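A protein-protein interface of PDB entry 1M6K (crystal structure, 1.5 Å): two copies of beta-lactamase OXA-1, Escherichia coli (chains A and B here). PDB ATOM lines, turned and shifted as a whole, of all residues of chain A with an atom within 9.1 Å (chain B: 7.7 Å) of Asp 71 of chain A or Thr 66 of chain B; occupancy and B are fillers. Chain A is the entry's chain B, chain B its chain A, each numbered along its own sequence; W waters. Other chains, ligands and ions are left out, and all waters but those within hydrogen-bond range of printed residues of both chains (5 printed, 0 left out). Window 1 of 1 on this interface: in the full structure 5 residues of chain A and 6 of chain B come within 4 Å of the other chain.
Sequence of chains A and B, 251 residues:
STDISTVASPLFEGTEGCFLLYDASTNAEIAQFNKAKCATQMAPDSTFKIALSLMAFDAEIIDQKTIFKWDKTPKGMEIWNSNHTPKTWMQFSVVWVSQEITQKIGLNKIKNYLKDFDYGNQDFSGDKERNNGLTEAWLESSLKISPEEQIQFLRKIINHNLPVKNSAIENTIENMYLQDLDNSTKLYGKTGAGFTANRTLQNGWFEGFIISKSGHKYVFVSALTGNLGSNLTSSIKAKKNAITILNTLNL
Of the 16 printed residues of chain B, 6 touch a printed residue of chain A.
Among the printed residues, Asp or Glu carboxylates within 4 Å of a Lys or Arg side-chain nitrogen of the other chain: Glu 100 of chain A with Lys 65 of chain B (2.6 Å).
The side-chain carboxylate of Asp 63 of chain B lies within hydrogen-bond range of the backbone NH of Lys 65 of chain B, at 2.9 Å.
N of Asp 63 of chain B lies within hydrogen-bond range of OG1 of Thr 66 of chain B.
NE1 of Trp 70 of chain A is in hydrogen-bond range of O of Thr 73 of chain A.
OG1 of Thr 73 of chain A lies within hydrogen-bond range of OD1 of Asp 71 of chain A (2.6 Å).
NZ of Lys 75 of chain A is in salt-bridge range of OD2 of Asp 71 of chain A (2.9 Å).
CD of Lys 72 of chain A touches O of Glu 60 of chain B, 3.4 Å away.
CB of Lys 72 of chain A touches O of Ile 61 of chain B, 3.4 Å away.
Lys 72 of chain A touches Ile 62 of chain B.
Lys 72 of chain A touches Asp 63 of chain B (CG to N, 3.98 Å).
CG2 of Thr 66 of chain B touches CG2 of Thr 73 of chain A, at 3.9 Å.
Water W5 lies within hydrogen-bond range of O of Lys 72 of chain A and O of Ile 61 of chain B.
Water W2 bridges OE2 of Glu 60 of chain B (2.8 Å) and NZ of Lys 72 of chain A (3.0 Å).
Water W1 lies within hydrogen-bond range of the side-chain carboxylate (OD2) of Asp 71 of chain A and the backbone carbonyl oxygen (O) of Lys 65 of chain B.
Water W4 lies within hydrogen-bond range of the side-chain carboxylate of Asp 71 of chain A, the backbone NH of Ile 67 of chain B and the side-chain hydroxyl of Thr 73 of chain A.
Water W3 lies within hydrogen-bond range of NZ of Lys 65 of chain B (2.9 Å), OE2 of Glu 100 of chain A (3.0 Å) and N of Lys 69 of chain A (3.1 Å).
Positions printed for both chains: 68, 69 and 84.
The side-chain amino group (NZ) of Lys 65 of chain B lies within hydrogen-bond range of the backbone carbonyl oxygen (O) of Lys 69 of chain A (2.8 Å).
The side-chain amino group of Lys 65 of chain B is in salt-bridge range of the side-chain carboxylate of Glu 100 of chain A (2.6 Å).
The side-chain hydroxyl of Thr 66 of chain B lies within hydrogen-bond range of the backbone carbonyl oxygen of Asp 71 of chain A (2.7 Å).
Asp 71 of chain A touches one residue of chain B.
Of chain A, only Asp 71 and Thr 73 come within 4 Å of Thr 66 of chain B.
Of the printed residues of chain B, Glu 100 of chain A touches Lys 65 (2.6 Å).
Of the printed residues of chain B, Lys 69 of chain A touches Lys 65.
Of the printed residues of chain A, Asp 63 of chain B touches Lys 72.
Of the printed residues of chain B, Thr 73 of chain A touches Thr 66.
Ile 67 of chain B touches none of the printed residues of chain A.
The nearest residue of chain B that does not touch Asp 71 of chain A is Lys 65 of chain B (4.2 Å).
The nearest printed residue of chain A that does not touch Ile 61 of chain B is Asp 71 of chain A (5.0 Å).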
ATOM      1  N   PHE A  68      -8.761  -4.505  21.666  1.00  0.00           N
ATOM      2  CA  PHE A  68      -9.902  -3.637  21.917  1.00  0.00           C
ATOM      3  C   PHE A  68      -9.676  -2.350  21.133  1.00  0.00           C
ATOM      4  O   PHE A  68      -8.665  -1.672  21.316  1.00  0.00           O
ATOM      5  CB  PHE A  68     -10.024  -3.350  23.419  1.00  0.00           C
ATOM      6  CG  PHE A  68     -10.083  -4.594  24.272  1.00  0.00           C
ATOM      7  CD1 PHE A  68      -8.961  -5.032  24.974  1.00  0.00           C
ATOM      8  CD2 PHE A  68     -11.258  -5.336  24.365  1.00  0.00           C
ATOM      9  CE1 PHE A  68      -9.009  -6.190  25.756  1.00  0.00           C
ATOM     10  CE2 PHE A  68     -11.316  -6.494  25.142  1.00  0.00           C
ATOM     11  CZ  PHE A  68     -10.190  -6.922  25.839  1.00  0.00           C
ATOM     12  N   LYS A  69     -10.623  -2.017  20.259  1.00  0.00           N
ATOM     13  CA  LYS A  69     -10.520  -0.835  19.410  1.00  0.00           C
ATOM     14  C   LYS A  69     -11.112   0.444  19.999  1.00  0.00           C
ATOM     15  O   LYS A  69     -12.277   0.479  20.395  1.00  0.00           O
ATOM     16  CB  LYS A  69     -11.184  -1.119  18.059  1.00  0.00           C
ATOM     17  CG  LYS A  69     -10.659  -2.363  17.352  1.00  0.00           C
ATOM     18  CD  LYS A  69      -9.175  -2.248  17.035  1.00  0.00           C
ATOM     19  CE  LYS A  69      -8.654  -3.517  16.372  1.00  0.00           C
ATOM     20  NZ  LYS A  69      -9.355  -3.801  15.089  1.00  0.00           N
ATOM     21  N   TRP A  70     -10.300   1.497  20.047  1.00  0.00           N
ATOM     22  CA  TRP A  70     -10.738   2.787  20.570  1.00  0.00           C
ATOM     23  C   TRP A  70     -11.747   3.394  19.597  1.00  0.00           C
ATOM     24  O   TRP A  70     -11.556   3.329  18.379  1.00  0.00           O
ATOM     25  CB  TRP A  70      -9.526   3.718  20.742  1.00  0.00           C
ATOM     26  CG  TRP A  70      -9.861   5.114  21.182  1.00  0.00           C
ATOM     27  CD1 TRP A  70     -10.710   5.476  22.190  1.00  0.00           C
ATOM     28  CD2 TRP A  70      -9.313   6.333  20.661  1.00  0.00           C
ATOM     29  NE1 TRP A  70     -10.724   6.845  22.331  1.00  0.00           N
ATOM     30  CE2 TRP A  70      -9.876   7.396  21.407  1.00  0.00           C
ATOM     31  CE3 TRP A  70      -8.400   6.633  19.638  1.00  0.00           C
ATOM     32  CZ2 TRP A  70      -9.556   8.736  21.163  1.00  0.00           C
ATOM     33  CZ3 TRP A  70      -8.083   7.971  19.395  1.00  0.00           C
ATOM     34  CH2 TRP A  70      -8.661   9.004  20.156  1.00  0.00           C
ATOM     35  N   ASP A  71     -12.814   3.982  20.135  1.00  0.00           N
ATOM     36  CA  ASP A  71     -13.857   4.589  19.307  1.00  0.00           C
ATOM     37  C   ASP A  71     -13.568   6.032  18.881  1.00  0.00           C
ATOM     38  O   ASP A  71     -14.458   6.728  18.393  1.00  0.00           O
ATOM     39  CB  ASP A  71     -15.215   4.530  20.022  1.00  0.00           C
ATOM     40  CG  ASP A  71     -15.235   5.317  21.322  1.00  0.00           C
ATOM     41  OD1 ASP A  71     -14.348   6.170  21.529  1.00  0.00           O
ATOM     42  OD2 ASP A  71     -16.159   5.089  22.133  1.00  0.00           O
ATOM     43  N   LYS A  72     -12.330   6.475  19.075  1.00  0.00           N
ATOM     44  CA  LYS A  72     -11.897   7.821  18.689  1.00  0.00           C
ATOM     45  C   LYS A  72     -12.436   8.985  19.523  1.00  0.00           C
ATOM     46  O   LYS A  72     -12.165  10.146  19.208  1.00  0.00           O
ATOM     47  CB  LYS A  72     -12.227   8.084  17.212  1.00  0.00           C
ATOM     48  CG  LYS A  72     -11.772   6.996  16.255  1.00  0.00           C
ATOM     49  CD  LYS A  72     -10.283   6.693  16.386  1.00  0.00           C
ATOM     50  CE  LYS A  72      -9.869   5.619  15.390  1.00  0.00           C
ATOM     51  NZ  LYS A  72      -8.432   5.257  15.496  1.00  0.00           N
ATOM     52  N   THR A  73     -13.197   8.695  20.572  1.00  0.00           N
ATOM     53  CA  THR A  73     -13.730   9.759  21.418  1.00  0.00           C
ATOM     54  C   THR A  73     -12.934   9.843  22.718  1.00  0.00           C
ATOM     55  O   THR A  73     -12.644   8.822  23.338  1.00  0.00           O
ATOM     56  CB  THR A  73     -15.212   9.525  21.770  1.00  0.00           C
ATOM     57  OG1 THR A  73     -15.342   8.312  22.519  1.00  0.00           O
ATOM     58  CG2 THR A  73     -16.052   9.427  20.506  1.00  0.00           C
ATOM     59  N   PRO A  74     -12.566  11.065  23.143  1.00  0.00           N
ATOM     60  CA  PRO A  74     -11.797  11.270  24.379  1.00  0.00           C
ATOM     61  C   PRO A  74     -12.415  10.556  25.578  1.00  0.00           C
ATOM     62  O   PRO A  74     -13.602  10.720  25.866  1.00  0.00           O
ATOM     63  CB  PRO A  74     -11.808  12.787  24.537  1.00  0.00           C
ATOM     64  CG  PRO A  74     -11.776  13.254  23.113  1.00  0.00           C
ATOM     65  CD  PRO A  74     -12.801  12.350  22.459  1.00  0.00           C
ATOM     66  N   LYS A  75     -11.600   9.778  26.285  1.00  0.00           N
ATOM     67  CA  LYS A  75     -12.072   9.022  27.439  1.00  0.00           C
ATOM     68  C   LYS A  75     -11.741   9.637  28.802  1.00  0.00           C
ATOM     69  O   LYS A  75     -12.183   9.129  29.833  1.00  0.00           O
ATOM     70  CB  LYS A  75     -11.529   7.591  27.366  1.00  0.00           C
ATOM     71  CG  LYS A  75     -11.964   6.827  26.123  1.00  0.00           C
ATOM     72  CD  LYS A  75     -13.469   6.593  26.117  1.00  0.00           C
ATOM     73  CE  LYS A  75     -13.910   5.867  24.856  1.00  0.00           C
ATOM     74  NZ  LYS A  75     -15.388   5.660  24.835  1.00  0.00           N
ATOM     75  N   TRP A  80      -5.863   6.110  27.717  1.00  0.00           N
ATOM     76  CA  TRP A  80      -7.065   5.348  27.381  1.00  0.00           C
ATOM     77  C   TRP A  80      -7.492   5.600  25.935  1.00  0.00           C
ATOM     78  O   TRP A  80      -8.261   4.823  25.369  1.00  0.00           O
ATOM     79  CB  TRP A  80      -8.241   5.725  28.290  1.00  0.00           C
ATOM     80  CG  TRP A  80      -8.104   5.319  29.728  1.00  0.00           C
ATOM     81  CD1 TRP A  80      -7.196   4.445  30.261  1.00  0.00           C
ATOM     82  CD2 TRP A  80      -8.947   5.733  30.814  1.00  0.00           C
ATOM     83  NE1 TRP A  80      -7.425   4.288  31.609  1.00  0.00           N
ATOM     84  CE2 TRP A  80      -8.494   5.067  31.973  1.00  0.00           C
ATOM     85  CE3 TRP A  80     -10.045   6.601  30.916  1.00  0.00           C
ATOM     86  CZ2 TRP A  80      -9.101   5.241  33.224  1.00  0.00           C
ATOM     87  CZ3 TRP A  80     -10.650   6.775  32.160  1.00  0.00           C
ATOM     88  CH2 TRP A  80     -10.174   6.097  33.296  1.00  0.00           C
ATOM     89  N   ASN A  81      -6.995   6.683  25.338  1.00  0.00           N
ATOM     90  CA  ASN A  81      -7.371   7.032  23.965  1.00  0.00           C
ATOM     91  C   ASN A  81      -6.511   6.329  22.927  1.00  0.00           C
ATOM     92  O   ASN A  81      -5.817   6.969  22.129  1.00  0.00           O
ATOM     93  CB  ASN A  81      -7.294   8.552  23.767  1.00  0.00           C
ATOM     94  CG  ASN A  81      -8.186   9.307  24.731  1.00  0.00           C
ATOM     95  OD1 ASN A  81      -9.246   8.819  25.121  1.00  0.00           O
ATOM     96  ND2 ASN A  81      -7.766  10.507  25.115  1.00  0.00           N
ATOM     97  N   SER A  82      -6.567   5.004  22.943  1.00  0.00           N
ATOM     98  CA  SER A  82      -5.798   4.185  22.022  1.00  0.00           C
ATOM     99  C   SER A  82      -6.289   2.744  22.089  1.00  0.00           C
ATOM    100  O   SER A  82      -7.127   2.403  22.929  1.00  0.00           O
ATOM    101  CB  SER A  82      -4.308   4.253  22.382  1.00  0.00           C
ATOM    102  OG  SER A  82      -4.086   3.893  23.737  1.00  0.00           O
ATOM    103  N   ASN A  83      -5.774   1.900  21.202  1.00  0.00           N
ATOM    104  CA  ASN A  83      -6.163   0.497  21.187  1.00  0.00           C
ATOM    105  C   ASN A  83      -5.468  -0.223  22.333  1.00  0.00           C
ATOM    106  O   ASN A  83      -4.355   0.138  22.715  1.00  0.00           O
ATOM    107  CB  ASN A  83      -5.792  -0.158  19.852  1.00  0.00           C
ATOM    108  CG  ASN A  83      -6.576   0.413  18.686  1.00  0.00           C
ATOM    109  OD1 ASN A  83      -7.608   1.063  18.873  1.00  0.00           O
ATOM    110  ND2 ASN A  83      -6.095   0.163  17.474  1.00  0.00           N
ATOM    111  N   HIS A  84      -6.128  -1.240  22.881  1.00  0.00           N
ATOM    112  CA  HIS A  84      -5.584  -1.994  24.004  1.00  0.00           C
ATOM    113  C   HIS A  84      -5.701  -3.504  23.846  1.00  0.00           C
ATOM    114  O   HIS A  84      -6.405  -3.997  22.965  1.00  0.00           O
ATOM    115  CB  HIS A  84      -6.285  -1.558  25.300  1.00  0.00           C
ATOM    116  CG  HIS A  84      -5.840  -0.219  25.792  1.00  0.00           C
ATOM    117  ND1 HIS A  84      -4.635  -0.031  26.433  1.00  0.00           N
ATOM    118  CD2 HIS A  84      -6.393   1.010  25.662  1.00  0.00           C
ATOM    119  CE1 HIS A  84      -4.462   1.256  26.673  1.00  0.00           C
ATOM    120  NE2 HIS A  84      -5.514   1.910  26.214  1.00  0.00           N
ATOM    121  N   TRP A  96     -13.111   1.749  29.871  1.00  0.00           N
ATOM    122  CA  TRP A  96     -14.002   1.478  28.741  1.00  0.00           C
ATOM    123  C   TRP A  96     -13.928   0.043  28.236  1.00  0.00           C
ATOM    124  O   TRP A  96     -14.910  -0.479  27.697  1.00  0.00           O
ATOM    125  CB  TRP A  96     -13.802   2.487  27.591  1.00  0.00           C
ATOM    126  CG  TRP A  96     -12.495   2.477  26.843  1.00  0.00           C
ATOM    127  CD1 TRP A  96     -11.452   3.353  27.000  1.00  0.00           C
ATOM    128  CD2 TRP A  96     -12.146   1.635  25.738  1.00  0.00           C
ATOM    129  NE1 TRP A  96     -10.485   3.115  26.051  1.00  0.00           N
ATOM    130  CE2 TRP A  96     -10.883   2.066  25.263  1.00  0.00           C
ATOM    131  CE3 TRP A  96     -12.779   0.562  25.093  1.00  0.00           C
ATOM    132  CZ2 TRP A  96     -10.243   1.459  24.175  1.00  0.00           C
ATOM    133  CZ3 TRP A  96     -12.140  -0.042  24.008  1.00  0.00           C
ATOM    134  CH2 TRP A  96     -10.883   0.410  23.561  1.00  0.00           C
ATOM    135  N   GLN A  99     -16.133  -1.980  30.488  1.00  0.00           N
ATOM    136  CA  GLN A  99     -17.532  -1.734  30.155  1.00  0.00           C
ATOM    137  C   GLN A  99     -17.975  -2.507  28.916  1.00  0.00           C
ATOM    138  O   GLN A  99     -19.132  -2.918  28.825  1.00  0.00           O
ATOM    139  CB  GLN A  99     -17.767  -0.233  29.992  1.00  0.00           C
ATOM    140  CG  GLN A  99     -17.433   0.541  31.266  1.00  0.00           C
ATOM    141  CD  GLN A  99     -17.526   2.037  31.090  1.00  0.00           C
ATOM    142  OE1 GLN A  99     -17.081   2.580  30.078  1.00  0.00           O
ATOM    143  NE2 GLN A  99     -18.087   2.719  32.083  1.00  0.00           N
ATOM    144  N   GLU A 100     -17.067  -2.715  27.967  1.00  0.00           N
ATOM    145  CA  GLU A 100     -17.409  -3.494  26.780  1.00  0.00           C
ATOM    146  C   GLU A 100     -17.603  -4.938  27.221  1.00  0.00           C
ATOM    147  O   GLU A 100     -18.503  -5.635  26.749  1.00  0.00           O
ATOM    148  CB  GLU A 100     -16.290  -3.440  25.735  1.00  0.00           C
ATOM    149  CG  GLU A 100     -16.274  -2.189  24.894  1.00  0.00           C
ATOM    150  CD  GLU A 100     -15.400  -2.328  23.656  1.00  0.00           C
ATOM    151  OE1 GLU A 100     -15.345  -1.372  22.862  1.00  0.00           O
ATOM    152  OE2 GLU A 100     -14.773  -3.394  23.475  1.00  0.00           O
ATOM    153  N   PHE B  57     -13.455   9.247   8.296  1.00  0.00           N
ATOM    154  CA  PHE B  57     -12.795   7.956   8.434  1.00  0.00           C
ATOM    155  C   PHE B  57     -11.316   8.067   8.064  1.00  0.00           C
ATOM    156  O   PHE B  57     -10.466   7.466   8.717  1.00  0.00           O
ATOM    157  CB  PHE B  57     -13.486   6.899   7.564  1.00  0.00           C
ATOM    158  CG  PHE B  57     -14.678   6.252   8.223  1.00  0.00           C
ATOM    159  CD1 PHE B  57     -14.504   5.370   9.286  1.00  0.00           C
ATOM    160  CD2 PHE B  57     -15.970   6.524   7.784  1.00  0.00           C
ATOM    161  CE1 PHE B  57     -15.601   4.768   9.904  1.00  0.00           C
ATOM    162  CE2 PHE B  57     -17.075   5.925   8.395  1.00  0.00           C
ATOM    163  CZ  PHE B  57     -16.889   5.046   9.456  1.00  0.00           C
ATOM    164  N   GLU B  60      -9.329   9.595  10.685  1.00  0.00           N
ATOM    165  CA  GLU B  60      -9.459   8.751  11.866  1.00  0.00           C
ATOM    166  C   GLU B  60     -10.097   9.436  13.073  1.00  0.00           C
ATOM    167  O   GLU B  60      -9.694   9.199  14.215  1.00  0.00           O
ATOM    168  CB  GLU B  60      -8.090   8.176  12.253  1.00  0.00           C
ATOM    169  CG  GLU B  60      -7.539   7.203  11.224  1.00  0.00           C
ATOM    170  CD  GLU B  60      -6.249   6.538  11.663  1.00  0.00           C
ATOM    171  OE1 GLU B  60      -5.745   5.682  10.908  1.00  0.00           O
ATOM    172  OE2 GLU B  60      -5.741   6.867  12.755  1.00  0.00           O
ATOM    173  N   ILE B  61     -11.095  10.283  12.832  1.00  0.00           N
ATOM    174  CA  ILE B  61     -11.767  10.949  13.942  1.00  0.00           C
ATOM    175  C   ILE B  61     -13.043  10.204  14.333  1.00  0.00           C
ATOM    176  O   ILE B  61     -13.692  10.547  15.319  1.00  0.00           O
ATOM    177  CB  ILE B  61     -12.086  12.430  13.636  1.00  0.00           C
ATOM    178  CG1 ILE B  61     -12.944  12.547  12.379  1.00  0.00           C
ATOM    179  CG2 ILE B  61     -10.787  13.216  13.488  1.00  0.00           C
ATOM    180  CD1 ILE B  61     -13.386  13.966  12.086  1.00  0.00           C
ATOM    181  N   ILE B  62     -13.408   9.200  13.540  1.00  0.00           N
ATOM    182  CA  ILE B  62     -14.562   8.364  13.860  1.00  0.00           C
ATOM    183  C   ILE B  62     -14.236   6.928  13.484  1.00  0.00           C
ATOM    184  O   ILE B  62     -13.340   6.668  12.675  1.00  0.00           O
ATOM    185  CB  ILE B  62     -15.873   8.776  13.115  1.00  0.00           C
ATOM    186  CG1 ILE B  62     -15.728   8.571  11.607  1.00  0.00           C
ATOM    187  CG2 ILE B  62     -16.238  10.207  13.448  1.00  0.00           C
ATOM    188  CD1 ILE B  62     -17.033   8.757  10.842  1.00  0.00           C
ATOM    189  N   ASP B  63     -14.963   6.004  14.100  1.00  0.00           N
ATOM    190  CA  ASP B  63     -14.823   4.575  13.868  1.00  0.00           C
ATOM    191  C   ASP B  63     -16.257   4.082  13.743  1.00  0.00           C
ATOM    192  O   ASP B  63     -17.185   4.788  14.146  1.00  0.00           O
ATOM    193  CB  ASP B  63     -14.159   3.906  15.078  1.00  0.00           C
ATOM    194  CG  ASP B  63     -13.916   2.423  14.867  1.00  0.00           C
ATOM    195  OD1 ASP B  63     -12.905   2.067  14.225  1.00  0.00           O
ATOM    196  OD2 ASP B  63     -14.741   1.609  15.337  1.00  0.00           O
ATOM    197  N   GLN B  64     -16.451   2.889  13.191  1.00  0.00           N
ATOM    198  CA  GLN B  64     -17.801   2.349  13.063  1.00  0.00           C
ATOM    199  C   GLN B  64     -18.442   2.189  14.444  1.00  0.00           C
ATOM    200  O   GLN B  64     -19.668   2.174  14.562  1.00  0.00           O
ATOM    201  CB  GLN B  64     -17.775   1.001  12.333  1.00  0.00           C
ATOM    202  CG  GLN B  64     -17.463   1.109  10.844  1.00  0.00           C
ATOM    203  CD  GLN B  64     -18.642   1.625  10.026  1.00  0.00           C
ATOM    204  OE1 GLN B  64     -19.307   2.587  10.405  1.00  0.00           O
ATOM    205  NE2 GLN B  64     -18.893   0.989   8.889  1.00  0.00           N
ATOM    206  N   LYS B  65     -17.608   2.089  15.483  1.00  0.00           N
ATOM    207  CA  LYS B  65     -18.073   1.930  16.868  1.00  0.00           C
ATOM    208  C   LYS B  65     -18.417   3.252  17.555  1.00  0.00           C
ATOM    209  O   LYS B  65     -18.974   3.259  18.653  1.00  0.00           O
ATOM    210  CB  LYS B  65     -16.999   1.239  17.722  1.00  0.00           C
ATOM    211  CG  LYS B  65     -16.679  -0.195  17.351  1.00  0.00           C
ATOM    212  CD  LYS B  65     -15.472  -0.710  18.142  1.00  0.00           C
ATOM    213  CE  LYS B  65     -15.668  -0.597  19.653  1.00  0.00           C
ATOM    214  NZ  LYS B  65     -14.495  -1.148  20.404  1.00  0.00           N
ATOM    215  N   THR B  66     -18.081   4.369  16.918  1.00  0.00           N
ATOM    216  CA  THR B  66     -18.329   5.678  17.508  1.00  0.00           C
ATOM    217  C   THR B  66     -19.801   5.998  17.749  1.00  0.00           C
ATOM    218  O   THR B  66     -20.644   5.752  16.893  1.00  0.00           O
ATOM    219  CB  THR B  66     -17.721   6.791  16.629  1.00  0.00           C
ATOM    220  OG1 THR B  66     -16.326   6.530  16.435  1.00  0.00           O
ATOM    221  CG2 THR B  66     -17.886   8.153  17.294  1.00  0.00           C
ATOM    222  N   ILE B  67     -20.100   6.535  18.930  1.00  0.00           N
ATOM    223  CA  ILE B  67     -21.464   6.927  19.271  1.00  0.00           C
ATOM    224  C   ILE B  67     -21.497   8.441  19.473  1.00  0.00           C
ATOM    225  O   ILE B  67     -20.812   8.978  20.349  1.00  0.00           O
ATOM    226  CB  ILE B  67     -21.961   6.244  20.569  1.00  0.00           C
ATOM    227  CG1 ILE B  67     -22.076   4.735  20.350  1.00  0.00           C
ATOM    228  CG2 ILE B  67     -23.318   6.822  20.975  1.00  0.00           C
ATOM    229  CD1 ILE B  67     -22.483   3.960  21.587  1.00  0.00           C
ATOM    230  N   PHE B  68     -22.278   9.132  18.649  1.00  0.00           N
ATOM    231  CA  PHE B  68     -22.404  10.579  18.762  1.00  0.00           C
ATOM    232  C   PHE B  68     -23.486  10.874  19.801  1.00  0.00           C
ATOM    233  O   PHE B  68     -24.628  10.438  19.656  1.00  0.00           O
ATOM    234  CB  PHE B  68     -22.794  11.193  17.411  1.00  0.00           C
ATOM    235  CG  PHE B  68     -21.868  10.824  16.281  1.00  0.00           C
ATOM    236  CD1 PHE B  68     -22.233   9.852  15.352  1.00  0.00           C
ATOM    237  CD2 PHE B  68     -20.633  11.449  16.143  1.00  0.00           C
ATOM    238  CE1 PHE B  68     -21.381   9.510  14.301  1.00  0.00           C
ATOM    239  CE2 PHE B  68     -19.772  11.113  15.093  1.00  0.00           C
ATOM    240  CZ  PHE B  68     -20.149  10.141  14.172  1.00  0.00           C
ATOM    241  N   LYS B  69     -23.119  11.615  20.844  1.00  0.00           N
ATOM    242  CA  LYS B  69     -24.040  11.946  21.932  1.00  0.00           C
ATOM    243  C   LYS B  69     -24.855  13.223  21.727  1.00  0.00           C
ATOM    244  O   LYS B  69     -24.298  14.310  21.591  1.00  0.00           O
ATOM    245  CB  LYS B  69     -23.263  12.070  23.247  1.00  0.00           C
ATOM    246  CG  LYS B  69     -22.388  10.873  23.588  1.00  0.00           C
ATOM    247  CD  LYS B  69     -23.212   9.631  23.880  1.00  0.00           C
ATOM    248  CE  LYS B  69     -22.318   8.463  24.276  1.00  0.00           C
ATOM    249  NZ  LYS B  69     -23.100   7.249  24.643  1.00  0.00           N
ATOM    250  N   HIS B  84     -26.561   8.897  17.936  1.00  0.00           N
ATOM    251  CA  HIS B  84     -26.414   8.309  16.610  1.00  0.00           C
ATOM    252  C   HIS B  84     -25.073   7.626  16.383  1.00  0.00           C
ATOM    253  O   HIS B  84     -24.149   7.760  17.181  1.00  0.00           O
ATOM    254  CB  HIS B  84     -26.631   9.400  15.553  1.00  0.00           C
ATOM    255  CG  HIS B  84     -28.071   9.770  15.370  1.00  0.00           C
ATOM    256  ND1 HIS B  84     -28.940   9.005  14.624  1.00  0.00           N
ATOM    257  CD2 HIS B  84     -28.807  10.781  15.888  1.00  0.00           C
ATOM    258  CE1 HIS B  84     -30.152   9.527  14.692  1.00  0.00           C
ATOM    259  NE2 HIS B  84     -30.100  10.604  15.454  1.00  0.00           N
ATOM    260  N   THR B  85     -24.989   6.877  15.290  1.00  0.00           N
ATOM    261  CA  THR B  85     -23.771   6.169  14.905  1.00  0.00           C
ATOM    262  C   THR B  85     -23.419   6.637  13.496  1.00  0.00           C
ATOM    263  O   THR B  85     -24.191   7.363  12.871  1.00  0.00           O
ATOM    264  CB  THR B  85     -23.994   4.651  14.848  1.00  0.00           C
ATOM    265  OG1 THR B  85     -24.859   4.337  13.746  1.00  0.00           O
ATOM    266  CG2 THR B  85     -24.626   4.158  16.144  1.00  0.00           C
ATOM    267  N   PRO B  86     -22.248   6.240  12.978  1.00  0.00           N
ATOM    268  CA  PRO B  86     -21.923   6.686  11.619  1.00  0.00           C
ATOM    269  C   PRO B  86     -22.960   6.192  10.608  1.00  0.00           C
ATOM    270  O   PRO B  86     -23.171   6.812   9.565  1.00  0.00           O
ATOM    271  CB  PRO B  86     -20.537   6.085  11.384  1.00  0.00           C
ATOM    272  CG  PRO B  86     -19.931   6.142  12.758  1.00  0.00           C
ATOM    273  CD  PRO B  86     -21.072   5.629  13.625  1.00  0.00           C
ATOM    274  N   LYS B  87     -23.609   5.072  10.918  1.00  0.00           N
ATOM    275  CA  LYS B  87     -24.624   4.525  10.031  1.00  0.00           C
ATOM    276  C   LYS B  87     -25.924   5.323  10.087  1.00  0.00           C
ATOM    277  O   LYS B  87     -26.462   5.696   9.044  1.00  0.00           O
ATOM    278  CB  LYS B  87     -24.905   3.055  10.372  1.00  0.00           C
ATOM    279  CG  LYS B  87     -23.790   2.104   9.958  1.00  0.00           C
ATOM    280  CD  LYS B  87     -24.148   0.660  10.298  1.00  0.00           C
ATOM    281  CE  LYS B  87     -23.032  -0.295   9.906  1.00  0.00           C
ATOM    282  NZ  LYS B  87     -22.758  -0.286   8.446  1.00  0.00           N
ATOM    283  N   THR B  88     -26.428   5.598  11.291  1.00  0.00           N
ATOM    284  CA  THR B  88     -27.683   6.340  11.399  1.00  0.00           C
ATOM    285  C   THR B  88     -27.513   7.816  11.033  1.00  0.00           C
ATOM    286  O   THR B  88     -28.478   8.488  10.679  1.00  0.00           O
ATOM    287  CB  THR B  88     -28.338   6.186  12.808  1.00  0.00           C
ATOM    288  OG1 THR B  88     -27.517   6.789  13.814  1.00  0.00           O
ATOM    289  CG2 THR B  88     -28.520   4.703  13.138  1.00  0.00           C
HETATM  290  O   HOH W   1     -18.344   3.469  21.666  1.00  0.00           O
HETATM  291  O   HOH W   2      -6.354   7.420  15.385  1.00  0.00           O
HETATM  292  O   HOH W   3     -13.150  -3.678  20.983  1.00  0.00           O
HETATM  293  O   HOH W   4     -18.135   6.919  21.136  1.00  0.00           O
HETATM  294  O   HOH W   5     -12.884  11.991  17.440  1.00  0.00           O
